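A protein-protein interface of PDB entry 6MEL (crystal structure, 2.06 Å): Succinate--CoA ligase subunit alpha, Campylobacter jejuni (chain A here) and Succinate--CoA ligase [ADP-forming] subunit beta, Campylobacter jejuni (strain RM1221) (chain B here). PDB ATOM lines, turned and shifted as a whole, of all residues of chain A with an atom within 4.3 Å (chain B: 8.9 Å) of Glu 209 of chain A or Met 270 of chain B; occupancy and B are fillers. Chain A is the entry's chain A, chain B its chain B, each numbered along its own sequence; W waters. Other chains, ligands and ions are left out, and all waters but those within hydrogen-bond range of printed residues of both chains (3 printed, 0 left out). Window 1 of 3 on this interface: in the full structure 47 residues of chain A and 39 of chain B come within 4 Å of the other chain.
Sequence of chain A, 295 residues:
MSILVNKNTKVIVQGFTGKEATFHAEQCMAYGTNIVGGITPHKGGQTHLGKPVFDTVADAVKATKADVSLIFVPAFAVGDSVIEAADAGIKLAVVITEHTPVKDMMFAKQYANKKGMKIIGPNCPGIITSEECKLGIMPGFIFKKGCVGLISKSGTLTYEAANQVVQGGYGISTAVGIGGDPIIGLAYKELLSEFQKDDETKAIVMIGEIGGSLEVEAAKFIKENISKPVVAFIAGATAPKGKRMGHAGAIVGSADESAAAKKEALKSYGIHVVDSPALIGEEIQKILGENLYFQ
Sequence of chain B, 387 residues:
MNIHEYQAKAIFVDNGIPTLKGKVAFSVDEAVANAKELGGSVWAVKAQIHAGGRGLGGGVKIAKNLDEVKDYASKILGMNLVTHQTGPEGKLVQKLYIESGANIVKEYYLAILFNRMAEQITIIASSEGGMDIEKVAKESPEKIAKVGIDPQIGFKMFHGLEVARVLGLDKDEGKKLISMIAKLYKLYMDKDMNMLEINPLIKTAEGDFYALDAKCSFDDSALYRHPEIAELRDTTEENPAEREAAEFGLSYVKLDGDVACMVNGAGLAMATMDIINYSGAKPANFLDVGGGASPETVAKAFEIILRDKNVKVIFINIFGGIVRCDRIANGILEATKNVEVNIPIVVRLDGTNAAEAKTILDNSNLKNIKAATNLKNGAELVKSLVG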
ATOM      1  N   LYS A 153      18.140  -8.152  25.031  1.00  0.00           N
ATOM      2  CA  LYS A 153      19.355  -8.389  24.287  1.00  0.00           C
ATOM      3  C   LYS A 153      20.598  -8.123  25.157  1.00  0.00           C
ATOM      4  O   LYS A 153      21.766  -8.299  24.663  1.00  0.00           O
ATOM      5  CB  LYS A 153      19.439  -7.463  23.080  1.00  0.00           C
ATOM      6  CG  LYS A 153      18.743  -7.897  21.794  1.00  0.00           C
ATOM      7  CD  LYS A 153      18.884  -6.828  20.745  1.00  0.00           C
ATOM      8  CE  LYS A 153      18.274  -7.239  19.428  1.00  0.00           C
ATOM      9  NZ  LYS A 153      18.433  -6.179  18.408  1.00  0.00           N
ATOM     10  N   SER A 154      20.409  -7.735  26.424  1.00  0.00           N
ATOM     11  CA  SER A 154      21.578  -7.462  27.281  1.00  0.00           C
ATOM     12  C   SER A 154      21.586  -8.284  28.580  1.00  0.00           C
ATOM     13  O   SER A 154      20.673  -9.091  28.853  1.00  0.00           O
ATOM     14  CB  SER A 154      21.790  -5.997  27.530  1.00  0.00           C
ATOM     15  OG  SER A 154      20.628  -5.261  27.462  1.00  0.00           O
ATOM     16  N   GLY A 208      15.814  -3.704  24.088  1.00  0.00           N
ATOM     17  CA  GLY A 208      16.522  -3.875  22.859  1.00  0.00           C
ATOM     18  C   GLY A 208      17.713  -2.966  22.800  1.00  0.00           C
ATOM     19  O   GLY A 208      18.041  -2.301  23.796  1.00  0.00           O
ATOM     20  N   GLU A 209      18.341  -2.951  21.626  1.00  0.00           N
ATOM     21  CA  GLU A 209      19.425  -2.059  21.339  1.00  0.00           C
ATOM     22  C   GLU A 209      19.583  -1.882  19.829  1.00  0.00           C
ATOM     23  O   GLU A 209      18.920  -2.547  19.039  1.00  0.00           O
ATOM     24  CB  GLU A 209      20.709  -2.520  22.029  1.00  0.00           C
ATOM     25  CG  GLU A 209      21.228  -3.867  21.616  1.00  0.00           C
ATOM     26  CD  GLU A 209      22.283  -4.472  22.548  1.00  0.00           C
ATOM     27  OE1 GLU A 209      22.094  -4.418  23.767  1.00  0.00           O
ATOM     28  OE2 GLU A 209      23.294  -5.018  22.024  1.00  0.00           O
ATOM     29  N   ILE A 210      20.454  -0.943  19.469  1.00  0.00           N
ATOM     30  CA  ILE A 210      20.835  -0.661  18.108  1.00  0.00           C
ATOM     31  C   ILE A 210      21.243  -1.953  17.403  1.00  0.00           C
ATOM     32  O   ILE A 210      21.791  -2.878  18.013  1.00  0.00           O
ATOM     33  CB  ILE A 210      21.974   0.359  18.059  1.00  0.00           C
ATOM     34  CG1 ILE A 210      23.154  -0.064  18.930  1.00  0.00           C
ATOM     35  CG2 ILE A 210      21.480   1.743  18.438  1.00  0.00           C
ATOM     36  CD1 ILE A 210      24.454   0.639  18.514  1.00  0.00           C
ATOM     37  N   GLY A 211      21.003  -1.969  16.084  1.00  0.00           N
ATOM     38  CA  GLY A 211      21.520  -3.030  15.189  1.00  0.00           C
ATOM     39  C   GLY A 211      20.410  -3.963  14.753  1.00  0.00           C
ATOM     40  O   GLY A 211      19.638  -4.476  15.593  1.00  0.00           O
ATOM     41  N   GLU A 215      13.335  -5.193  16.513  1.00  0.00           N
ATOM     42  CA  GLU A 215      12.417  -4.425  17.363  1.00  0.00           C
ATOM     43  C   GLU A 215      11.398  -3.648  16.498  1.00  0.00           C
ATOM     44  O   GLU A 215      10.271  -3.423  16.932  1.00  0.00           O
ATOM     45  CB  GLU A 215      13.210  -3.513  18.311  1.00  0.00           C
ATOM     46  CG  GLU A 215      14.137  -4.264  19.265  1.00  0.00           C
ATOM     47  CD  GLU A 215      15.558  -4.442  18.758  1.00  0.00           C
ATOM     48  OE1 GLU A 215      15.761  -4.441  17.517  1.00  0.00           O
ATOM     49  OE2 GLU A 215      16.471  -4.551  19.592  1.00  0.00           O
ATOM     50  N   ILE A 234      14.902   0.822  24.363  1.00  0.00           N
ATOM     51  CA  ILE A 234      15.821   0.540  23.304  1.00  0.00           C
ATOM     52  C   ILE A 234      17.087   1.331  23.598  1.00  0.00           C
ATOM     53  O   ILE A 234      17.084   2.518  23.459  1.00  0.00           O
ATOM     54  CB  ILE A 234      15.273   0.917  21.906  1.00  0.00           C
ATOM     55  CG1 ILE A 234      13.886   0.327  21.631  1.00  0.00           C
ATOM     56  CG2 ILE A 234      16.276   0.491  20.828  1.00  0.00           C
ATOM     57  CD1 ILE A 234      13.799  -1.197  21.773  1.00  0.00           C
ATOM     58  N   ALA A 235      18.174   0.636  23.946  1.00  0.00           N
ATOM     59  CA  ALA A 235      19.439   1.313  24.268  1.00  0.00           C
ATOM     60  C   ALA A 235      20.153   1.792  22.998  1.00  0.00           C
ATOM     61  O   ALA A 235      20.110   1.143  21.958  1.00  0.00           O
ATOM     62  CB  ALA A 235      20.303   0.333  25.003  1.00  0.00           C
ATOM     63  N   GLY A 236      20.874   2.908  23.104  1.00  0.00           N
ATOM     64  CA  GLY A 236      21.759   3.359  22.015  1.00  0.00           C
ATOM     65  C   GLY A 236      21.285   4.608  21.275  1.00  0.00           C
ATOM     66  O   GLY A 236      21.796   4.892  20.214  1.00  0.00           O
ATOM     67  N   MET A 245      29.207  -0.895  19.616  1.00  0.00           N
ATOM     68  CA  MET A 245      29.077  -0.515  21.020  1.00  0.00           C
ATOM     69  C   MET A 245      29.120  -1.777  21.907  1.00  0.00           C
ATOM     70  O   MET A 245      28.110  -2.266  22.445  1.00  0.00           O
ATOM     71  CB  MET A 245      27.801   0.296  21.206  1.00  0.00           C
ATOM     72  CG  MET A 245      27.683   1.458  20.168  1.00  0.00           C
ATOM     73  SD  MET A 245      29.071   2.706  20.242  1.00  0.00           S
ATOM     74  CE  MET A 245      28.522   3.356  21.794  1.00  0.00           C
ATOM     75  N   HIS A 247      28.792  -5.033  22.153  1.00  0.00           N
ATOM     76  CA  HIS A 247      28.196  -6.229  21.509  1.00  0.00           C
ATOM     77  C   HIS A 247      28.454  -6.272  19.995  1.00  0.00           C
ATOM     78  O   HIS A 247      28.237  -5.284  19.254  1.00  0.00           O
ATOM     79  CB  HIS A 247      26.681  -6.205  21.690  1.00  0.00           C
ATOM     80  CG  HIS A 247      26.221  -6.559  23.045  1.00  0.00           C
ATOM     81  ND1 HIS A 247      24.981  -6.194  23.461  1.00  0.00           N
ATOM     82  CD2 HIS A 247      26.782  -7.307  24.025  1.00  0.00           C
ATOM     83  CE1 HIS A 247      24.790  -6.661  24.675  1.00  0.00           C
ATOM     84  NE2 HIS A 247      25.873  -7.395  25.042  1.00  0.00           N
ATOM     85  N   ALA A 250      25.694  -4.722  18.104  1.00  0.00           N
ATOM     86  CA  ALA A 250      25.267  -3.376  18.439  1.00  0.00           C
ATOM     87  C   ALA A 250      25.988  -2.363  17.557  1.00  0.00           C
ATOM     88  O   ALA A 250      26.901  -1.674  18.011  1.00  0.00           O
ATOM     89  CB  ALA A 250      25.491  -3.085  19.903  1.00  0.00           C
ATOM     90  N   LYS A 262      13.596   2.417  15.962  1.00  0.00           N
ATOM     91  CA  LYS A 262      12.934   1.339  16.645  1.00  0.00           C
ATOM     92  C   LYS A 262      11.880   1.909  17.604  1.00  0.00           C
ATOM     93  O   LYS A 262      10.757   1.401  17.706  1.00  0.00           O
ATOM     94  CB  LYS A 262      13.965   0.510  17.429  1.00  0.00           C
ATOM     95  CG  LYS A 262      14.919  -0.221  16.513  1.00  0.00           C
ATOM     96  CD  LYS A 262      16.047  -0.970  17.181  1.00  0.00           C
ATOM     97  CE  LYS A 262      16.921  -1.588  16.110  1.00  0.00           C
ATOM     98  NZ  LYS A 262      17.666  -2.735  16.643  1.00  0.00           N
ATOM     99  N   ARG B 116      21.773  -9.558   7.601  1.00  0.00           N
ATOM    100  CA  ARG B 116      21.465  -9.828   9.006  1.00  0.00           C
ATOM    101  C   ARG B 116      20.011 -10.272   9.139  1.00  0.00           C
ATOM    102  O   ARG B 116      19.736 -11.272   9.810  1.00  0.00           O
ATOM    103  CB  ARG B 116      21.804  -8.591   9.859  1.00  0.00           C
ATOM    104  CG  ARG B 116      21.526  -8.768  11.344  1.00  0.00           C
ATOM    105  CD  ARG B 116      22.088  -7.631  12.174  1.00  0.00           C
ATOM    106  NE  ARG B 116      21.564  -7.700  13.527  1.00  0.00           N
ATOM    107  CZ  ARG B 116      22.045  -7.005  14.538  1.00  0.00           C
ATOM    108  NH1 ARG B 116      23.069  -6.189  14.322  1.00  0.00           N
ATOM    109  NH2 ARG B 116      21.509  -7.164  15.740  1.00  0.00           N
ATOM    110  N   VAL B 253      34.838   3.545  23.357  1.00  0.00           N
ATOM    111  CA  VAL B 253      34.620   4.342  22.193  1.00  0.00           C
ATOM    112  C   VAL B 253      34.597   5.790  22.675  1.00  0.00           C
ATOM    113  O   VAL B 253      33.801   6.118  23.602  1.00  0.00           O
ATOM    114  CB  VAL B 253      33.297   3.997  21.474  1.00  0.00           C
ATOM    115  CG1 VAL B 253      33.069   4.918  20.300  1.00  0.00           C
ATOM    116  CG2 VAL B 253      33.231   2.539  21.027  1.00  0.00           C
ATOM    117  N   LEU B 255      33.496   9.657  22.375  1.00  0.00           N
ATOM    118  CA  LEU B 255      32.549  10.629  21.838  1.00  0.00           C
ATOM    119  C   LEU B 255      33.018  12.056  22.206  1.00  0.00           C
ATOM    120  O   LEU B 255      34.061  12.232  22.800  1.00  0.00           O
ATOM    121  CB  LEU B 255      31.166  10.353  22.439  1.00  0.00           C
ATOM    122  CG  LEU B 255      30.309   9.282  21.755  1.00  0.00           C
ATOM    123  CD1 LEU B 255      30.854   7.912  22.013  1.00  0.00           C
ATOM    124  CD2 LEU B 255      28.863   9.363  22.246  1.00  0.00           C
ATOM    125  N   CYS B 261      31.796   7.983  31.228  1.00  0.00           N
ATOM    126  CA  CYS B 261      31.084   6.943  31.880  1.00  0.00           C
ATOM    127  C   CYS B 261      31.941   5.665  31.993  1.00  0.00           C
ATOM    128  O   CYS B 261      32.915   5.428  31.258  1.00  0.00           O
ATOM    129  CB  CYS B 261      29.668   6.898  31.298  1.00  0.00           C
ATOM    130  SG  CYS B 261      29.401   5.779  29.917  1.00  0.00           S
ATOM    131  N   VAL B 263      30.935   1.633  33.040  1.00  0.00           N
ATOM    132  CA  VAL B 263      29.749   0.802  33.241  1.00  0.00           C
ATOM    133  C   VAL B 263      30.087  -0.667  32.961  1.00  0.00           C
ATOM    134  O   VAL B 263      30.947  -0.980  32.121  1.00  0.00           O
ATOM    135  CB  VAL B 263      28.624   1.281  32.297  1.00  0.00           C
ATOM    136  CG1 VAL B 263      27.351   0.501  32.500  1.00  0.00           C
ATOM    137  CG2 VAL B 263      28.361   2.795  32.345  1.00  0.00           C
ATOM    138  N   ASN B 264      29.370  -1.592  33.590  1.00  0.00           N
ATOM    139  CA  ASN B 264      29.553  -2.982  33.249  1.00  0.00           C
ATOM    140  C   ASN B 264      28.390  -3.469  32.351  1.00  0.00           C
ATOM    141  O   ASN B 264      27.209  -3.425  32.744  1.00  0.00           O
ATOM    142  CB  ASN B 264      29.764  -3.858  34.488  1.00  0.00           C
ATOM    143  CG  ASN B 264      28.598  -3.963  35.454  1.00  0.00           C
ATOM    144  OD1 ASN B 264      27.843  -2.992  35.640  1.00  0.00           O
ATOM    145  ND2 ASN B 264      28.517  -5.118  36.130  1.00  0.00           N
ATOM    146  N   GLY B 265      28.755  -3.966  31.160  1.00  0.00           N
ATOM    147  CA  GLY B 265      27.824  -4.541  30.185  1.00  0.00           C
ATOM    148  C   GLY B 265      27.457  -3.496  29.122  1.00  0.00           C
ATOM    149  O   GLY B 265      27.163  -2.334  29.433  1.00  0.00           O
ATOM    150  N   ALA B 266      27.491  -3.913  27.867  1.00  0.00           N
ATOM    151  CA  ALA B 266      27.346  -3.019  26.728  1.00  0.00           C
ATOM    152  C   ALA B 266      25.957  -2.370  26.737  1.00  0.00           C
ATOM    153  O   ALA B 266      25.861  -1.212  26.417  1.00  0.00           O
ATOM    154  CB  ALA B 266      27.607  -3.757  25.431  1.00  0.00           C
ATOM    155  N   GLY B 267      24.912  -3.143  27.048  1.00  0.00           N
ATOM    156  CA  GLY B 267      23.590  -2.621  27.072  1.00  0.00           C
ATOM    157  C   GLY B 267      23.444  -1.521  28.116  1.00  0.00           C
ATOM    158  O   GLY B 267      22.910  -0.420  27.840  1.00  0.00           O
ATOM    159  N   LEU B 268      23.918  -1.810  29.333  1.00  0.00           N
ATOM    160  CA  LEU B 268      23.815  -0.825  30.412  1.00  0.00           C
ATOM    161  C   LEU B 268      24.728   0.365  30.119  1.00  0.00           C
ATOM    162  O   LEU B 268      24.412   1.510  30.480  1.00  0.00           O
ATOM    163  CB  LEU B 268      24.164  -1.479  31.743  1.00  0.00           C
ATOM    164  CG  LEU B 268      24.045  -0.595  32.980  1.00  0.00           C
ATOM    165  CD1 LEU B 268      22.581  -0.243  33.246  1.00  0.00           C
ATOM    166  CD2 LEU B 268      24.587  -1.330  34.208  1.00  0.00           C
ATOM    167  N   ALA B 269      25.870   0.123  29.472  1.00  0.00           N
ATOM    168  CA  ALA B 269      26.769   1.235  29.117  1.00  0.00           C
ATOM    169  C   ALA B 269      26.073   2.191  28.130  1.00  0.00           C
ATOM    170  O   ALA B 269      26.142   3.398  28.326  1.00  0.00           O
ATOM    171  CB  ALA B 269      28.079   0.754  28.563  1.00  0.00           C
ATOM    172  N   MET B 270      25.441   1.646  27.081  1.00  0.00           N
ATOM    173  CA  MET B 270      24.633   2.454  26.102  1.00  0.00           C
ATOM    174  C   MET B 270      23.522   3.190  26.873  1.00  0.00           C
ATOM    175  O   MET B 270      23.296   4.362  26.677  1.00  0.00           O
ATOM    176  CB  MET B 270      24.020   1.581  24.984  1.00  0.00           C
ATOM    177  CG  MET B 270      24.996   1.331  23.860  1.00  0.00           C
ATOM    178  SD  MET B 270      24.319   0.347  22.498  1.00  0.00           S
ATOM    179  CE  MET B 270      24.387  -1.310  23.149  1.00  0.00           C
ATOM    180  N   ALA B 271      22.821   2.484  27.762  1.00  0.00           N
ATOM    181  CA  ALA B 271      21.719   3.088  28.512  1.00  0.00           C
ATOM    182  C   ALA B 271      22.215   4.242  29.382  1.00  0.00           C
ATOM    183  O   ALA B 271      21.457   5.170  29.604  1.00  0.00           O
ATOM    184  CB  ALA B 271      21.013   2.077  29.361  1.00  0.00           C
ATOM    185  N   THR B 272      23.444   4.130  29.902  1.00  0.00           N
ATOM    186  CA  THR B 272      24.067   5.149  30.727  1.00  0.00           C
ATOM    187  C   THR B 272      24.368   6.387  29.883  1.00  0.00           C
ATOM    188  O   THR B 272      24.077   7.531  30.300  1.00  0.00           O
ATOM    189  CB  THR B 272      25.304   4.620  31.451  1.00  0.00           C
ATOM    190  OG1 THR B 272      24.943   3.501  32.276  1.00  0.00           O
ATOM    191  CG2 THR B 272      25.937   5.691  32.306  1.00  0.00           C
ATOM    192  N   MET B 273      24.927   6.178  28.696  1.00  0.00           N
ATOM    193  CA  MET B 273      25.119   7.280  27.771  1.00  0.00           C
ATOM    194  C   MET B 273      23.765   7.945  27.478  1.00  0.00           C
ATOM    195  O   MET B 273      23.685   9.193  27.440  1.00  0.00           O
ATOM    196  CB  MET B 273      25.729   6.805  26.456  1.00  0.00           C
ATOM    197  CG  MET B 273      27.088   6.150  26.625  1.00  0.00           C
ATOM    198  SD  MET B 273      27.551   5.256  25.108  1.00  0.00           S
ATOM    199  CE  MET B 273      27.574   6.596  23.920  1.00  0.00           C
ATOM    200  N   ASP B 274      22.714   7.128  27.326  1.00  0.00           N
ATOM    201  CA  ASP B 274      21.400   7.630  26.975  1.00  0.00           C
ATOM    202  C   ASP B 274      20.828   8.470  28.119  1.00  0.00           C
ATOM    203  O   ASP B 274      20.340   9.553  27.856  1.00  0.00           O
ATOM    204  CB  ASP B 274      20.420   6.533  26.584  1.00  0.00           C
ATOM    205  CG  ASP B 274      20.829   5.745  25.351  1.00  0.00           C
ATOM    206  OD1 ASP B 274      21.708   6.246  24.563  1.00  0.00           O
ATOM    207  OD2 ASP B 274      20.245   4.632  25.171  1.00  0.00           O
ATOM    208  N   ILE B 275      20.930   8.007  29.372  1.00  0.00           N
ATOM    209  CA  ILE B 275      20.400   8.769  30.487  1.00  0.00           C
ATOM    210  C   ILE B 275      21.183  10.080  30.717  1.00  0.00           C
ATOM    211  O   ILE B 275      20.621  11.061  31.176  1.00  0.00           O
ATOM    212  CB  ILE B 275      20.273   7.933  31.773  1.00  0.00           C
ATOM    213  CG1 ILE B 275      19.165   8.506  32.650  1.00  0.00           C
ATOM    214  CG2 ILE B 275      21.601   7.827  32.511  1.00  0.00           C
ATOM    215  CD1 ILE B 275      18.824   7.650  33.835  1.00  0.00           C
ATOM    216  N   ILE B 276      22.466  10.118  30.391  1.00  0.00           N
ATOM    217  CA  ILE B 276      23.216  11.347  30.533  1.00  0.00           C
ATOM    218  C   ILE B 276      22.598  12.373  29.571  1.00  0.00           C
ATOM    219  O   ILE B 276      22.364  13.489  29.974  1.00  0.00           O
ATOM    220  CB  ILE B 276      24.718  11.099  30.267  1.00  0.00           C
ATOM    221  CG1 ILE B 276      25.383  10.329  31.406  1.00  0.00           C
ATOM    222  CG2 ILE B 276      25.464  12.382  29.973  1.00  0.00           C
ATOM    223  CD1 ILE B 276      26.733   9.695  31.015  1.00  0.00           C
ATOM    224  N   ASN B 277      22.338  11.960  28.313  1.00  0.00           N
ATOM    225  CA  ASN B 277      21.696  12.808  27.291  1.00  0.00           C
ATOM    226  C   ASN B 277      20.304  13.245  27.758  1.00  0.00           C
ATOM    227  O   ASN B 277      19.957  14.410  27.717  1.00  0.00           O
ATOM    228  CB  ASN B 277      21.593  12.135  25.924  1.00  0.00           C
ATOM    229  CG  ASN B 277      20.948  13.039  24.885  1.00  0.00           C
ATOM    230  OD1 ASN B 277      21.464  14.106  24.568  1.00  0.00           O
ATOM    231  ND2 ASN B 277      19.799  12.642  24.387  1.00  0.00           N
ATOM    232  N   PRO B 283      27.248  12.480  26.806  1.00  0.00           N
ATOM    233  CA  PRO B 283      28.232  11.445  27.095  1.00  0.00           C
ATOM    234  C   PRO B 283      29.558  11.631  26.338  1.00  0.00           C
ATOM    235  O   PRO B 283      29.580  11.870  25.120  1.00  0.00           O
ATOM    236  CB  PRO B 283      27.518  10.152  26.706  1.00  0.00           C
ATOM    237  CG  PRO B 283      26.447  10.599  25.707  1.00  0.00           C
ATOM    238  CD  PRO B 283      26.030  11.988  26.142  1.00  0.00           C
ATOM    239  N   ASN B 285      31.943   9.268  26.262  1.00  0.00           N
ATOM    240  CA  ASN B 285      32.495   7.974  25.880  1.00  0.00           C
ATOM    241  C   ASN B 285      31.488   6.865  26.186  1.00  0.00           C
ATOM    242  O   ASN B 285      30.584   7.021  27.011  1.00  0.00           O
ATOM    243  CB  ASN B 285      33.822   7.673  26.596  1.00  0.00           C
ATOM    244  CG  ASN B 285      33.600   7.306  28.054  1.00  0.00           C
ATOM    245  OD1 ASN B 285      33.268   8.179  28.829  1.00  0.00           O
ATOM    246  ND2 ASN B 285      33.714   6.035  28.433  1.00  0.00           N
ATOM    247  N   PHE B 286      31.696   5.734  25.512  1.00  0.00           N
ATOM    248  CA  PHE B 286      31.198   4.418  25.865  1.00  0.00           C
ATOM    249  C   PHE B 286      32.360   3.695  26.536  1.00  0.00           C
ATOM    250  O   PHE B 286      33.506   3.748  26.019  1.00  0.00           O
ATOM    251  CB  PHE B 286      30.757   3.663  24.603  1.00  0.00           C
ATOM    252  CG  PHE B 286      30.455   2.198  24.756  1.00  0.00           C
ATOM    253  CD1 PHE B 286      31.462   1.261  24.683  1.00  0.00           C
ATOM    254  CD2 PHE B 286      29.169   1.746  24.984  1.00  0.00           C
ATOM    255  CE1 PHE B 286      31.196  -0.096  24.793  1.00  0.00           C
ATOM    256  CE2 PHE B 286      28.906   0.389  25.108  1.00  0.00           C
ATOM    257  CZ  PHE B 286      29.918  -0.529  25.040  1.00  0.00           C
ATOM    258  N   LEU B 287      32.110   3.068  27.685  1.00  0.00           N
ATOM    259  CA  LEU B 287      33.106   2.148  28.278  1.00  0.00           C
ATOM    260  C   LEU B 287      32.379   1.032  29.022  1.00  0.00           C
ATOM    261  O   LEU B 287      31.563   1.307  29.935  1.00  0.00           O
ATOM    262  CB  LEU B 287      34.051   2.875  29.236  1.00  0.00           C
ATOM    263  CG  LEU B 287      34.911   1.914  30.062  1.00  0.00           C
ATOM    264  CD1 LEU B 287      35.939   1.266  29.189  1.00  0.00           C
ATOM    265  CD2 LEU B 287      35.598   2.603  31.193  1.00  0.00           C
ATOM    266  N   ASP B 288      32.690  -0.201  28.612  1.00  0.00           N
ATOM    267  CA  ASP B 288      32.260  -1.402  29.224  1.00  0.00           C
ATOM    268  C   ASP B 288      33.473  -2.031  29.923  1.00  0.00           C
ATOM    269  O   ASP B 288      34.453  -2.385  29.293  1.00  0.00           O
ATOM    270  CB  ASP B 288      31.602  -2.338  28.208  1.00  0.00           C
ATOM    271  CG  ASP B 288      31.368  -3.767  28.678  1.00  0.00           C
ATOM    272  OD1 ASP B 288      31.313  -4.004  29.904  1.00  0.00           O
ATOM    273  OD2 ASP B 288      31.254  -4.655  27.790  1.00  0.00           O
ATOM    274  N   ASN B 317      28.498   3.534  36.756  1.00  0.00           N
ATOM    275  CA  ASN B 317      27.199   2.935  36.874  1.00  0.00           C
ATOM    276  C   ASN B 317      27.421   1.439  36.738  1.00  0.00           C
ATOM    277  O   ASN B 317      27.698   0.949  35.651  1.00  0.00           O
ATOM    278  CB  ASN B 317      26.222   3.489  35.838  1.00  0.00           C
ATOM    279  CG  ASN B 317      24.868   2.798  35.884  1.00  0.00           C
ATOM    280  OD1 ASN B 317      24.497   2.252  36.914  1.00  0.00           O
ATOM    281  ND2 ASN B 317      24.136   2.790  34.781  1.00  0.00           N
HETATM  282  O   HOH W   1      19.892  -8.975  16.989  1.00  0.00           O
HETATM  283  O   HOH W   2      21.173  -5.547  18.094  1.00  0.00           O
HETATM  284  O   HOH W   3      17.948   4.834  24.149  1.00  0.00           O
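A ring nitrogen (ND1) of His 247 of chain A lies within hydrogen-bond range of the side-chain carboxylate (OE2) of Glu 209 of chain A (2.5 Å). O of Val 253 of chain B is in hydrogen-bond range of N of Phe 286 of chain B, 2.9 Å away. The side-chain carboxylate of Glu 215 of chain A sits at hydrogen-bond distance from the backbone NH of Glu 209 of chain A (3.2 Å). O of Glu 209 of chain A sits at hydrogen-bond distance from NZ of Lys 262 of chain A. The backbone NH (N) of Ala 235 of chain A sits at hydrogen-bond distance from the backbone carbonyl oxygen (O) of Gly 208 of chain A, 2.9 Å away. O of Gly 211 of chain A sits at hydrogen-bond distance from NZ of Lys 262 of chain A (2.8 Å).
CB of Ser 154 of chain A touches CA of Gly 267 of chain B, at 3.9 Å. Met 270 of chain B touches Glu 209 of chain A. CG1 of Ile 210 of chain A touches SD of Met 270 of chain B, 3.8 Å away. CB of Ala 235 of chain A touches O of Gly 267 of chain B, 3.9 Å away. Ala 235 of chain A touches Asp 274 of chain B. Met 270 of chain B touches Gly 236 of chain A. CB of Met 245 of chain A touches SD of Met 270 of chain B, 3.7 Å away. CE of Met 245 of chain A touches SD of Met 273 of chain B, 3.9 Å away. His 247 of chain A touches Ala 266 of chain B. Met 270 of chain B touches Ala 250 of chain A (CE to CB, 3.9 Å).
Hydrophobic or aromatic side chains of chain B within 4 Å of the printed part of chain A: Ala 266, Met 270, Met 273 and Phe 286. Hydrophobic or aromatic side chains of chain A that line the printed part of chain B: Ile 210, Ala 235, Met 245, His 247 and Ala 250. Among the printed residues, 15 pairs touch across the chains.
The backbone NH of Gly 236 of chain A lies within hydrogen-bond range of the side-chain carboxylate of Asp 274 of chain B, 2.8 Å away. The guanidinium group (NH2) of Arg 116 of chain B lies within hydrogen-bond range of the backbone carbonyl oxygen (O) of Gly 211 of chain A (3.3 Å).
Glu 209 of chain A touches just one residue of chain B: Met 270. Of chain B, only Met 270 (3.8 Å) comes within 4 Å of Ile 210 of chain A. Gly 211 of chain A touches one residue of chain B. Of chain B, only Gly 267 (3.9 Å), Met 270 (3.9 Å) and Asp 274 (3.5 Å) come within 4 Å of Ala 235 of chain A. Of the printed residues of chain B, Gly 236 of chain A touches Met 270 and Asp 274. Printed residues of chain A within 4 Å of Gly 267 of chain B: Ser 154 (3.9 Å) and Ala 235 (3.9 Å). Of chain A, only Glu 209, Ile 210, Ala 235, Gly 236, Met 245 and Ala 250 come within 4 Å of Met 270 of chain B. Of the printed residues of chain A, Met 273 of chain B touches Met 245 (3.9 Å). Printed residues of chain A within 4 Å of Asp 274 of chain B: Ala 235 (3.5 Å) and Gly 236 (2.8 Å). Of the printed residues of chain A, Phe 286 of chain B touches Met 245. The nearest residue of chain B that does not touch Glu 209 of chain A is Gly 267 of chain B (4.05 Å).
Water W3 bridges the side-chain carboxylate of Asp 274 of chain B and the backbone carbonyl oxygen of Ile 234 of chain A. Water W1 bridges the guanidinium group of Arg 116 of chain B (2.7 Å) and the side-chain amino group of Lys 153 of chain A (3.5 Å). Water W2 lies within hydrogen-bond range of the backbone carbonyl oxygen (O) of Ile 210 of chain A, the side-chain amino group (NZ) of Lys 153 of chain A, the guanidinium group (NH2) of Arg 116 of chain B and the backbone carbonyl oxygen (O) of Gly 211 of chain A.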
